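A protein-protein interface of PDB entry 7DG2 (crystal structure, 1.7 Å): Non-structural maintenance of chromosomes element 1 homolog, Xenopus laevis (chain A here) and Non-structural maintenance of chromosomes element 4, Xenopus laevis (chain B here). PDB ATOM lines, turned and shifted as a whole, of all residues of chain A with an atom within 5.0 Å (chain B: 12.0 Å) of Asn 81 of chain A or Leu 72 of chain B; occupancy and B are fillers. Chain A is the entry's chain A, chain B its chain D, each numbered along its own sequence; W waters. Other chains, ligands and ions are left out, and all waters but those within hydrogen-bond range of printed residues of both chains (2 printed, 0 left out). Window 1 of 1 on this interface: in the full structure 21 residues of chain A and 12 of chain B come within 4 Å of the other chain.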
ATOM      1  N   PHE A  61      -9.688  -8.379 -19.568  1.00  0.00           N
ATOM      2  CA  PHE A  61      -8.839  -7.393 -20.240  1.00  0.00           C
ATOM      3  C   PHE A  61      -7.701  -6.934 -19.338  1.00  0.00           C
ATOM      4  O   PHE A  61      -7.375  -5.748 -19.262  1.00  0.00           O
ATOM      5  CB  PHE A  61      -9.670  -6.209 -20.727  1.00  0.00           C
ATOM      6  CG  PHE A  61     -10.746  -6.613 -21.688  1.00  0.00           C
ATOM      7  CD1 PHE A  61     -10.423  -7.008 -22.975  1.00  0.00           C
ATOM      8  CD2 PHE A  61     -12.069  -6.620 -21.301  1.00  0.00           C
ATOM      9  CE1 PHE A  61     -11.413  -7.394 -23.866  1.00  0.00           C
ATOM     10  CE2 PHE A  61     -13.066  -7.004 -22.191  1.00  0.00           C
ATOM     11  CZ  PHE A  61     -12.739  -7.390 -23.465  1.00  0.00           C
ATOM     12  N   MET A  62      -7.105  -7.897 -18.639  1.00  0.00           N
ATOM     13  CA  MET A  62      -5.930  -7.707 -17.807  1.00  0.00           C
ATOM     14  C   MET A  62      -4.894  -8.747 -18.227  1.00  0.00           C
ATOM     15  O   MET A  62      -5.249  -9.845 -18.663  1.00  0.00           O
ATOM     16  CB  MET A  62      -6.281  -7.877 -16.312  1.00  0.00           C
ATOM     17  CG  MET A  62      -7.394  -6.936 -15.839  1.00  0.00           C
ATOM     18  SD  MET A  62      -7.996  -7.424 -14.204  1.00  0.00           S
ATOM     19  CE  MET A  62      -6.476  -7.351 -13.303  1.00  0.00           C
ATOM     20  N   LEU A  79       1.342  -5.895 -14.268  1.00  0.00           N
ATOM     21  CA  LEU A  79      -0.082  -6.151 -14.441  1.00  0.00           C
ATOM     22  C   LEU A  79      -0.672  -4.948 -15.169  1.00  0.00           C
ATOM     23  O   LEU A  79      -0.687  -3.839 -14.622  1.00  0.00           O
ATOM     24  CB  LEU A  79      -0.765  -6.359 -13.088  1.00  0.00           C
ATOM     25  CG  LEU A  79      -2.276  -6.610 -13.178  1.00  0.00           C
ATOM     26  CD1 LEU A  79      -2.568  -7.925 -13.936  1.00  0.00           C
ATOM     27  CD2 LEU A  79      -2.878  -6.659 -11.771  1.00  0.00           C
ATOM     28  N   VAL A  80      -1.127  -5.154 -16.402  1.00  0.00           N
ATOM     29  CA  VAL A  80      -1.555  -4.039 -17.241  1.00  0.00           C
ATOM     30  C   VAL A  80      -3.006  -4.227 -17.666  1.00  0.00           C
ATOM     31  O   VAL A  80      -3.510  -5.346 -17.814  1.00  0.00           O
ATOM     32  CB  VAL A  80      -0.632  -3.860 -18.475  1.00  0.00           C
ATOM     33  CG1 VAL A  80       0.780  -3.541 -18.016  1.00  0.00           C
ATOM     34  CG2 VAL A  80      -0.628  -5.094 -19.359  1.00  0.00           C
ATOM     35  N   ASN A  81      -3.683  -3.100 -17.842  1.00  0.00           N
ATOM     36  CA  ASN A  81      -5.010  -3.081 -18.418  1.00  0.00           C
ATOM     37  C   ASN A  81      -4.911  -3.114 -19.939  1.00  0.00           C
ATOM     38  O   ASN A  81      -3.958  -2.601 -20.530  1.00  0.00           O
ATOM     39  CB  ASN A  81      -5.746  -1.828 -17.960  1.00  0.00           C
ATOM     40  CG  ASN A  81      -7.122  -1.739 -18.539  1.00  0.00           C
ATOM     41  OD1 ASN A  81      -7.852  -2.726 -18.555  1.00  0.00           O
ATOM     42  ND2 ASN A  81      -7.483  -0.563 -19.044  1.00  0.00           N
ATOM     43  N   ARG A  82      -5.903  -3.728 -20.579  1.00  0.00           N
ATOM     44  CA  ARG A  82      -5.813  -3.950 -22.016  1.00  0.00           C
ATOM     45  C   ARG A  82      -7.057  -3.489 -22.771  1.00  0.00           C
ATOM     46  O   ARG A  82      -7.224  -3.852 -23.940  1.00  0.00           O
ATOM     47  CB  ARG A  82      -5.512  -5.428 -22.298  1.00  0.00           C
ATOM     48  CG  ARG A  82      -4.004  -5.759 -22.183  1.00  0.00           C
ATOM     49  CD  ARG A  82      -3.271  -5.068 -23.336  1.00  0.00           C
ATOM     50  NE  ARG A  82      -1.809  -4.958 -23.234  1.00  0.00           N
ATOM     51  CZ  ARG A  82      -1.162  -3.881 -22.781  1.00  0.00           C
ATOM     52  NH1 ARG A  82      -1.839  -2.819 -22.334  1.00  0.00           N
ATOM     53  NH2 ARG A  82       0.173  -3.861 -22.777  1.00  0.00           N
ATOM     54  N   VAL A  83      -7.924  -2.678 -22.160  1.00  0.00           N
ATOM     55  CA  VAL A  83      -9.132  -2.225 -22.846  1.00  0.00           C
ATOM     56  C   VAL A  83      -9.443  -0.780 -22.482  1.00  0.00           C
ATOM     57  O   VAL A  83      -9.139  -0.303 -21.383  1.00  0.00           O
ATOM     58  CB  VAL A  83     -10.343  -3.143 -22.540  1.00  0.00           C
ATOM     59  CG1 VAL A  83     -10.828  -2.931 -21.115  1.00  0.00           C
ATOM     60  CG2 VAL A  83     -11.465  -2.913 -23.543  1.00  0.00           C
ATOM     61  N   GLU A  84     -10.050  -0.066 -23.426  1.00  0.00           N
ATOM     62  CA  GLU A  84     -10.524   1.292 -23.189  1.00  0.00           C
ATOM     63  C   GLU A  84     -12.039   1.258 -23.348  1.00  0.00           C
ATOM     64  O   GLU A  84     -12.537   1.071 -24.460  1.00  0.00           O
ATOM     65  CB  GLU A  84      -9.862   2.276 -24.166  1.00  0.00           C
ATOM     66  CG  GLU A  84      -8.325   2.114 -24.236  1.00  0.00           C
ATOM     67  CD  GLU A  84      -7.660   2.822 -25.425  1.00  0.00           C
ATOM     68  OE1 GLU A  84      -7.539   4.066 -25.402  1.00  0.00           O
ATOM     69  OE2 GLU A  84      -7.244   2.123 -26.377  1.00  0.00           O
ATOM     70  N   THR A  88     -13.521   1.398 -17.655  1.00  0.00           N
ATOM     71  CA  THR A  88     -12.165   1.811 -17.299  1.00  0.00           C
ATOM     72  C   THR A  88     -12.093   3.316 -17.080  1.00  0.00           C
ATOM     73  O   THR A  88     -11.300   3.790 -16.260  1.00  0.00           O
ATOM     74  CB  THR A  88     -11.162   1.377 -18.370  1.00  0.00           C
ATOM     75  OG1 THR A  88     -11.497   1.975 -19.628  1.00  0.00           O
ATOM     76  CG2 THR A  88     -11.159  -0.131 -18.514  1.00  0.00           C
ATOM     77  N   GLU A 168       2.335  -0.768 -20.466  1.00  0.00           N
ATOM     78  CA  GLU A 168       0.882  -0.712 -20.607  1.00  0.00           C
ATOM     79  C   GLU A 168       0.452   0.079 -21.842  1.00  0.00           C
ATOM     80  O   GLU A 168      -0.530  -0.283 -22.505  1.00  0.00           O
ATOM     81  CB  GLU A 168       0.250  -0.104 -19.362  1.00  0.00           C
ATOM     82  CG  GLU A 168      -1.271  -0.201 -19.398  1.00  0.00           C
ATOM     83  CD  GLU A 168      -1.890   0.196 -18.084  1.00  0.00           C
ATOM     84  OE1 GLU A 168      -2.089   1.411 -17.864  1.00  0.00           O
ATOM     85  OE2 GLU A 168      -2.141  -0.711 -17.262  1.00  0.00           O
ATOM     86  N   LEU A 169       1.158   1.163 -22.161  1.00  0.00           N
ATOM     87  CA  LEU A 169       0.741   2.085 -23.212  1.00  0.00           C
ATOM     88  C   LEU A 169       1.459   1.860 -24.538  1.00  0.00           C
ATOM     89  O   LEU A 169       1.310   2.684 -25.446  1.00  0.00           O
ATOM     90  CB  LEU A 169       0.952   3.538 -22.767  1.00  0.00           C
ATOM     91  CG  LEU A 169       0.089   4.005 -21.588  1.00  0.00           C
ATOM     92  CD1 LEU A 169       0.237   5.514 -21.390  1.00  0.00           C
ATOM     93  CD2 LEU A 169      -1.341   3.677 -21.830  1.00  0.00           C
ATOM     94  N   TYR A 172      -1.025   1.873 -27.417  1.00  0.00           N
ATOM     95  CA  TYR A 172      -1.669   3.178 -27.414  1.00  0.00           C
ATOM     96  C   TYR A 172      -0.753   4.241 -28.016  1.00  0.00           C
ATOM     97  O   TYR A 172      -1.174   5.042 -28.859  1.00  0.00           O
ATOM     98  CB  TYR A 172      -2.066   3.538 -25.985  1.00  0.00           C
ATOM     99  CG  TYR A 172      -2.632   4.911 -25.835  1.00  0.00           C
ATOM    100  CD1 TYR A 172      -3.990   5.148 -26.008  1.00  0.00           C
ATOM    101  CD2 TYR A 172      -1.810   5.982 -25.524  1.00  0.00           C
ATOM    102  CE1 TYR A 172      -4.508   6.416 -25.867  1.00  0.00           C
ATOM    103  CE2 TYR A 172      -2.315   7.246 -25.387  1.00  0.00           C
ATOM    104  CZ  TYR A 172      -3.664   7.460 -25.555  1.00  0.00           C
ATOM    105  OH  TYR A 172      -4.152   8.731 -25.411  1.00  0.00           O
ATOM    106  N   THR B  67      -5.801  -3.187  -4.582  1.00  0.00           N
ATOM    107  CA  THR B  67      -6.670  -2.600  -5.592  1.00  0.00           C
ATOM    108  C   THR B  67      -5.930  -2.523  -6.924  1.00  0.00           C
ATOM    109  O   THR B  67      -4.693  -2.470  -6.970  1.00  0.00           O
ATOM    110  CB  THR B  67      -7.171  -1.196  -5.163  1.00  0.00           C
ATOM    111  OG1 THR B  67      -6.064  -0.381  -4.737  1.00  0.00           O
ATOM    112  CG2 THR B  67      -8.181  -1.312  -4.013  1.00  0.00           C
ATOM    113  N   PHE B  68      -6.702  -2.536  -8.007  1.00  0.00           N
ATOM    114  CA  PHE B  68      -6.183  -2.568  -9.371  1.00  0.00           C
ATOM    115  C   PHE B  68      -6.148  -1.157  -9.935  1.00  0.00           C
ATOM    116  O   PHE B  68      -7.173  -0.471  -9.948  1.00  0.00           O
ATOM    117  CB  PHE B  68      -7.061  -3.463 -10.245  1.00  0.00           C
ATOM    118  CG  PHE B  68      -6.663  -3.495 -11.703  1.00  0.00           C
ATOM    119  CD1 PHE B  68      -5.337  -3.650 -12.086  1.00  0.00           C
ATOM    120  CD2 PHE B  68      -7.634  -3.430 -12.682  1.00  0.00           C
ATOM    121  CE1 PHE B  68      -4.989  -3.706 -13.437  1.00  0.00           C
ATOM    122  CE2 PHE B  68      -7.295  -3.499 -14.038  1.00  0.00           C
ATOM    123  CZ  PHE B  68      -5.981  -3.635 -14.409  1.00  0.00           C
ATOM    124  N   HIS B  69      -4.974  -0.738 -10.400  1.00  0.00           N
ATOM    125  CA  HIS B  69      -4.769   0.603 -10.933  1.00  0.00           C
ATOM    126  C   HIS B  69      -4.088   0.512 -12.287  1.00  0.00           C
ATOM    127  O   HIS B  69      -3.296  -0.397 -12.538  1.00  0.00           O
ATOM    128  CB  HIS B  69      -3.937   1.447  -9.966  1.00  0.00           C
ATOM    129  CG  HIS B  69      -4.602   1.615  -8.636  1.00  0.00           C
ATOM    130  ND1 HIS B  69      -5.413   2.689  -8.336  1.00  0.00           N
ATOM    131  CD2 HIS B  69      -4.621   0.809  -7.547  1.00  0.00           C
ATOM    132  CE1 HIS B  69      -5.884   2.549  -7.107  1.00  0.00           C
ATOM    133  NE2 HIS B  69      -5.420   1.416  -6.609  1.00  0.00           N
ATOM    134  N   PHE B  70      -4.420   1.458 -13.164  1.00  0.00           N
ATOM    135  CA  PHE B  70      -3.948   1.424 -14.540  1.00  0.00           C
ATOM    136  C   PHE B  70      -4.057   2.842 -15.086  1.00  0.00           C
ATOM    137  O   PHE B  70      -4.712   3.707 -14.494  1.00  0.00           O
ATOM    138  CB  PHE B  70      -4.781   0.445 -15.378  1.00  0.00           C
ATOM    139  CG  PHE B  70      -6.256   0.685 -15.231  1.00  0.00           C
ATOM    140  CD1 PHE B  70      -6.897   1.644 -16.002  1.00  0.00           C
ATOM    141  CD2 PHE B  70      -6.979   0.023 -14.254  1.00  0.00           C
ATOM    142  CE1 PHE B  70      -8.250   1.908 -15.831  1.00  0.00           C
ATOM    143  CE2 PHE B  70      -8.335   0.277 -14.083  1.00  0.00           C
ATOM    144  CZ  PHE B  70      -8.967   1.229 -14.866  1.00  0.00           C
ATOM    145  N   MET B  71      -3.431   3.064 -16.235  1.00  0.00           N
ATOM    146  CA  MET B  71      -3.529   4.335 -16.946  1.00  0.00           C
ATOM    147  C   MET B  71      -4.296   4.207 -18.254  1.00  0.00           C
ATOM    148  O   MET B  71      -5.191   5.010 -18.529  1.00  0.00           O
ATOM    149  CB  MET B  71      -2.110   4.880 -17.205  1.00  0.00           C
ATOM    150  CG  MET B  71      -2.065   6.255 -17.853  1.00  0.00           C
ATOM    151  SD  MET B  71      -2.819   7.521 -16.817  1.00  0.00           S
ATOM    152  CE  MET B  71      -1.636   7.735 -15.483  1.00  0.00           C
ATOM    153  N   LEU B  72      -3.973   3.205 -19.071  1.00  0.00           N
ATOM    154  CA  LEU B  72      -4.686   2.979 -20.323  1.00  0.00           C
ATOM    155  C   LEU B  72      -6.183   2.845 -20.068  1.00  0.00           C
ATOM    156  O   LEU B  72      -6.607   2.089 -19.189  1.00  0.00           O
ATOM    157  CB  LEU B  72      -4.161   1.711 -21.001  1.00  0.00           C
ATOM    158  CG  LEU B  72      -4.932   1.278 -22.253  1.00  0.00           C
ATOM    159  CD1 LEU B  72      -4.617   2.230 -23.396  1.00  0.00           C
ATOM    160  CD2 LEU B  72      -4.603  -0.162 -22.646  1.00  0.00           C
ATOM    161  N   GLY B  73      -6.991   3.585 -20.837  1.00  0.00           N
ATOM    162  CA  GLY B  73      -8.431   3.497 -20.676  1.00  0.00           C
ATOM    163  C   GLY B  73      -9.005   4.349 -19.567  1.00  0.00           C
ATOM    164  O   GLY B  73     -10.235   4.384 -19.402  1.00  0.00           O
ATOM    165  N   SER B  74      -8.171   5.049 -18.807  1.00  0.00           N
ATOM    166  CA  SER B  74      -8.681   5.908 -17.751  1.00  0.00           C
ATOM    167  C   SER B  74      -9.024   7.307 -18.247  1.00  0.00           C
ATOM    168  O   SER B  74      -9.658   8.064 -17.507  1.00  0.00           O
ATOM    169  CB  SER B  74      -7.667   6.013 -16.609  1.00  0.00           C
ATOM    170  OG  SER B  74      -6.539   6.813 -16.975  1.00  0.00           O
ATOM    171  N   PHE B  75      -8.634   7.645 -19.478  1.00  0.00           N
ATOM    172  CA  PHE B  75      -8.782   9.000 -20.012  1.00  0.00           C
ATOM    173  C   PHE B  75     -10.209   9.235 -20.482  1.00  0.00           C
ATOM    174  O   PHE B  75     -10.769   8.408 -21.209  1.00  0.00           O
ATOM    175  CB  PHE B  75      -7.849   9.228 -21.204  1.00  0.00           C
ATOM    176  CG  PHE B  75      -6.402   8.948 -20.935  1.00  0.00           C
ATOM    177  CD1 PHE B  75      -5.843   9.199 -19.702  1.00  0.00           C
ATOM    178  CD2 PHE B  75      -5.593   8.447 -21.950  1.00  0.00           C
ATOM    179  CE1 PHE B  75      -4.491   8.951 -19.476  1.00  0.00           C
ATOM    180  CE2 PHE B  75      -4.255   8.190 -21.729  1.00  0.00           C
ATOM    181  CZ  PHE B  75      -3.702   8.445 -20.486  1.00  0.00           C
ATOM    182  N   LYS B  76     -10.776  10.382 -20.117  1.00  0.00           N
ATOM    183  CA  LYS B  76     -12.101  10.788 -20.596  1.00  0.00           C
ATOM    184  C   LYS B  76     -11.930  12.006 -21.502  1.00  0.00           C
ATOM    185  O   LYS B  76     -11.945  13.146 -21.035  1.00  0.00           O
ATOM    186  CB  LYS B  76     -13.053  11.093 -19.428  1.00  0.00           C
ATOM    187  CG  LYS B  76     -14.442  11.568 -19.875  1.00  0.00           C
ATOM    188  CD  LYS B  76     -14.977  12.697 -18.991  1.00  0.00           C
ATOM    189  CE  LYS B  76     -15.525  13.851 -19.834  1.00  0.00           C
ATOM    190  NZ  LYS B  76     -16.019  14.997 -19.011  1.00  0.00           N
ATOM    191  N   THR B  77     -11.766  11.768 -22.802  1.00  0.00           N
ATOM    192  CA  THR B  77     -11.679  10.430 -23.377  1.00  0.00           C
ATOM    193  C   THR B  77     -10.386  10.304 -24.181  1.00  0.00           C
ATOM    194  O   THR B  77      -9.560  11.215 -24.178  1.00  0.00           O
ATOM    195  CB  THR B  77     -12.885  10.111 -24.283  1.00  0.00           C
ATOM    196  OG1 THR B  77     -12.964  11.079 -25.338  1.00  0.00           O
ATOM    197  CG2 THR B  77     -14.182  10.136 -23.479  1.00  0.00           C
HETATM  198  O   HOH W   1      -1.597  -2.667 -12.290  1.00  0.00           O
HETATM  199  O   HOH W   2      -6.624   5.535 -22.607  1.00  0.00           O
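The backbone carbonyl oxygen of Leu 72 of chain B sits at hydrogen-bond distance from the side-chain amide nitrogen of Asn 81 of chain A, 2.8 Å away. The side-chain hydroxyl (OG1) of Thr 88 of chain A lies within hydrogen-bond range of the backbone carbonyl oxygen (O) of Gly 73 of chain B, 2.7 Å away. The side-chain carboxylate (OE1) of Glu 168 of chain A lies within hydrogen-bond range of the backbone NH (N) of Met 71 of chain B. OE1 of Glu 168 of chain A sits at hydrogen-bond distance from N of Leu 72 of chain B, 2.9 Å away.
OD1 of Asn 81 of chain A sits close to O of Phe 61 of chain A. N of Arg 82 of chain A sits at hydrogen-bond distance from O of Phe 61 of chain A, 2.8 Å away. The side-chain amide nitrogen (ND2) of Asn 81 of chain A is in hydrogen-bond range of the backbone carbonyl oxygen (O) of Val 83 of chain A, 2.9 Å away. N of Asn 81 of chain A lies within hydrogen-bond range of OE2 of Glu 168 of chain A (2.9 Å). O of Glu 168 of chain A lies within hydrogen-bond range of NH1 of Arg 82 of chain A, at 2.9 Å. The side-chain hydroxyl (OG) of Ser 74 of chain B is in hydrogen-bond range of the backbone carbonyl oxygen (O) of Met 71 of chain B (2.7 Å).
Among the printed residues, merely in contact across the chains: Glu 168 of chain A with Phe 70 of chain B (3.4 Å), Leu 169 of chain A with Leu 72 of chain B (3.5 Å), Asn 81 of chain A with Phe 70 of chain B (3.6 Å), Thr 88 of chain A with Phe 70 of chain B (3.6 Å), Thr 88 of chain A with Ser 74 of chain B (3.7 Å), Glu 84 of chain A with Leu 72 of chain B (3.7 Å), Tyr 172 of chain A with Phe 75 of chain B (3.7 Å), Glu 84 of chain A with Gly 73 of chain B (3.8 Å), Arg 82 of chain A with Leu 72 of chain B (3.8 Å), Tyr 172 of chain A with Leu 72 of chain B (3.9 Å), Met 62 of chain A with Phe 68 of chain B (3.9 Å), Leu 79 of chain A with Phe 68 of chain B (3.9 Å), Val 83 of chain A with Gly 73 of chain B (3.9 Å) and Asn 81 of chain A with Phe 68 of chain B (3.99 Å).
Met 62 of chain A touches one residue of chain B. No residue of chain B comes within 4 Å of Val 80 of chain A. Printed residues of chain B within 4 Å of Asn 81 of chain A: Phe 68, Phe 70 and Leu 72. Of chain B, only Leu 72 (3.8 Å) comes within 4 Å of Arg 82 of chain A. Of chain B, only Gly 73 comes within 4 Å of Val 83 of chain A. Glu 84 of chain A touches just these residues of chain B: Leu 72 and Gly 73. Thr 88 of chain A touches just these residues of chain B: Phe 70 (3.6 Å), Gly 73 (2.7 Å) and Ser 74 (3.7 Å). Leu 169 of chain A touches just one residue of chain B: Leu 72. His 69 of chain B touches none of the printed residues of chain A. Printed residues of chain A within 4 Å of Phe 70 of chain B: Asn 81, Thr 88 and Glu 168. Of the printed residues of chain A, Met 71 of chain B touches Glu 168 (2.7 Å). Leu 72 of chain B touches just these residues of chain A: Asn 81, Arg 82, Glu 84, Glu 168, Leu 169 and Tyr 172. Printed residues of chain A within 4 Å of Gly 73 of chain B: Val 83 (3.9 Å), Glu 84 (3.8 Å) and Thr 88 (2.7 Å). The nearest residue of chain A that does not touch Leu 72 of chain B is Val 83 of chain A (4.1 Å).
Of the 12 printed residues of chain A, 10 touch a printed residue of chain B. Along chain A the printed residues that touch a printed residue of chain B span positions 62 to 172. Printed residues of chain B that touch a printed residue of chain A: Phe 68, Phe 70, Met 71, Leu 72, Gly 73, Ser 74 and Phe 75. Among the printed residues, no Asp or Glu carboxylate lies within 4 Å of a Lys or Arg side-chain nitrogen of the other chain.
Water W2 bridges the backbone NH (N) of Gly 73 of chain B (2.7 Å) and the side-chain carboxylate (OE1) of Glu 84 of chain A (3.3 Å). Water W1 bridges the backbone carbonyl oxygen (O) of Leu 79 of chain A (2.8 Å) and the backbone carbonyl oxygen (O) of His 69 of chain B (2.8 Å).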
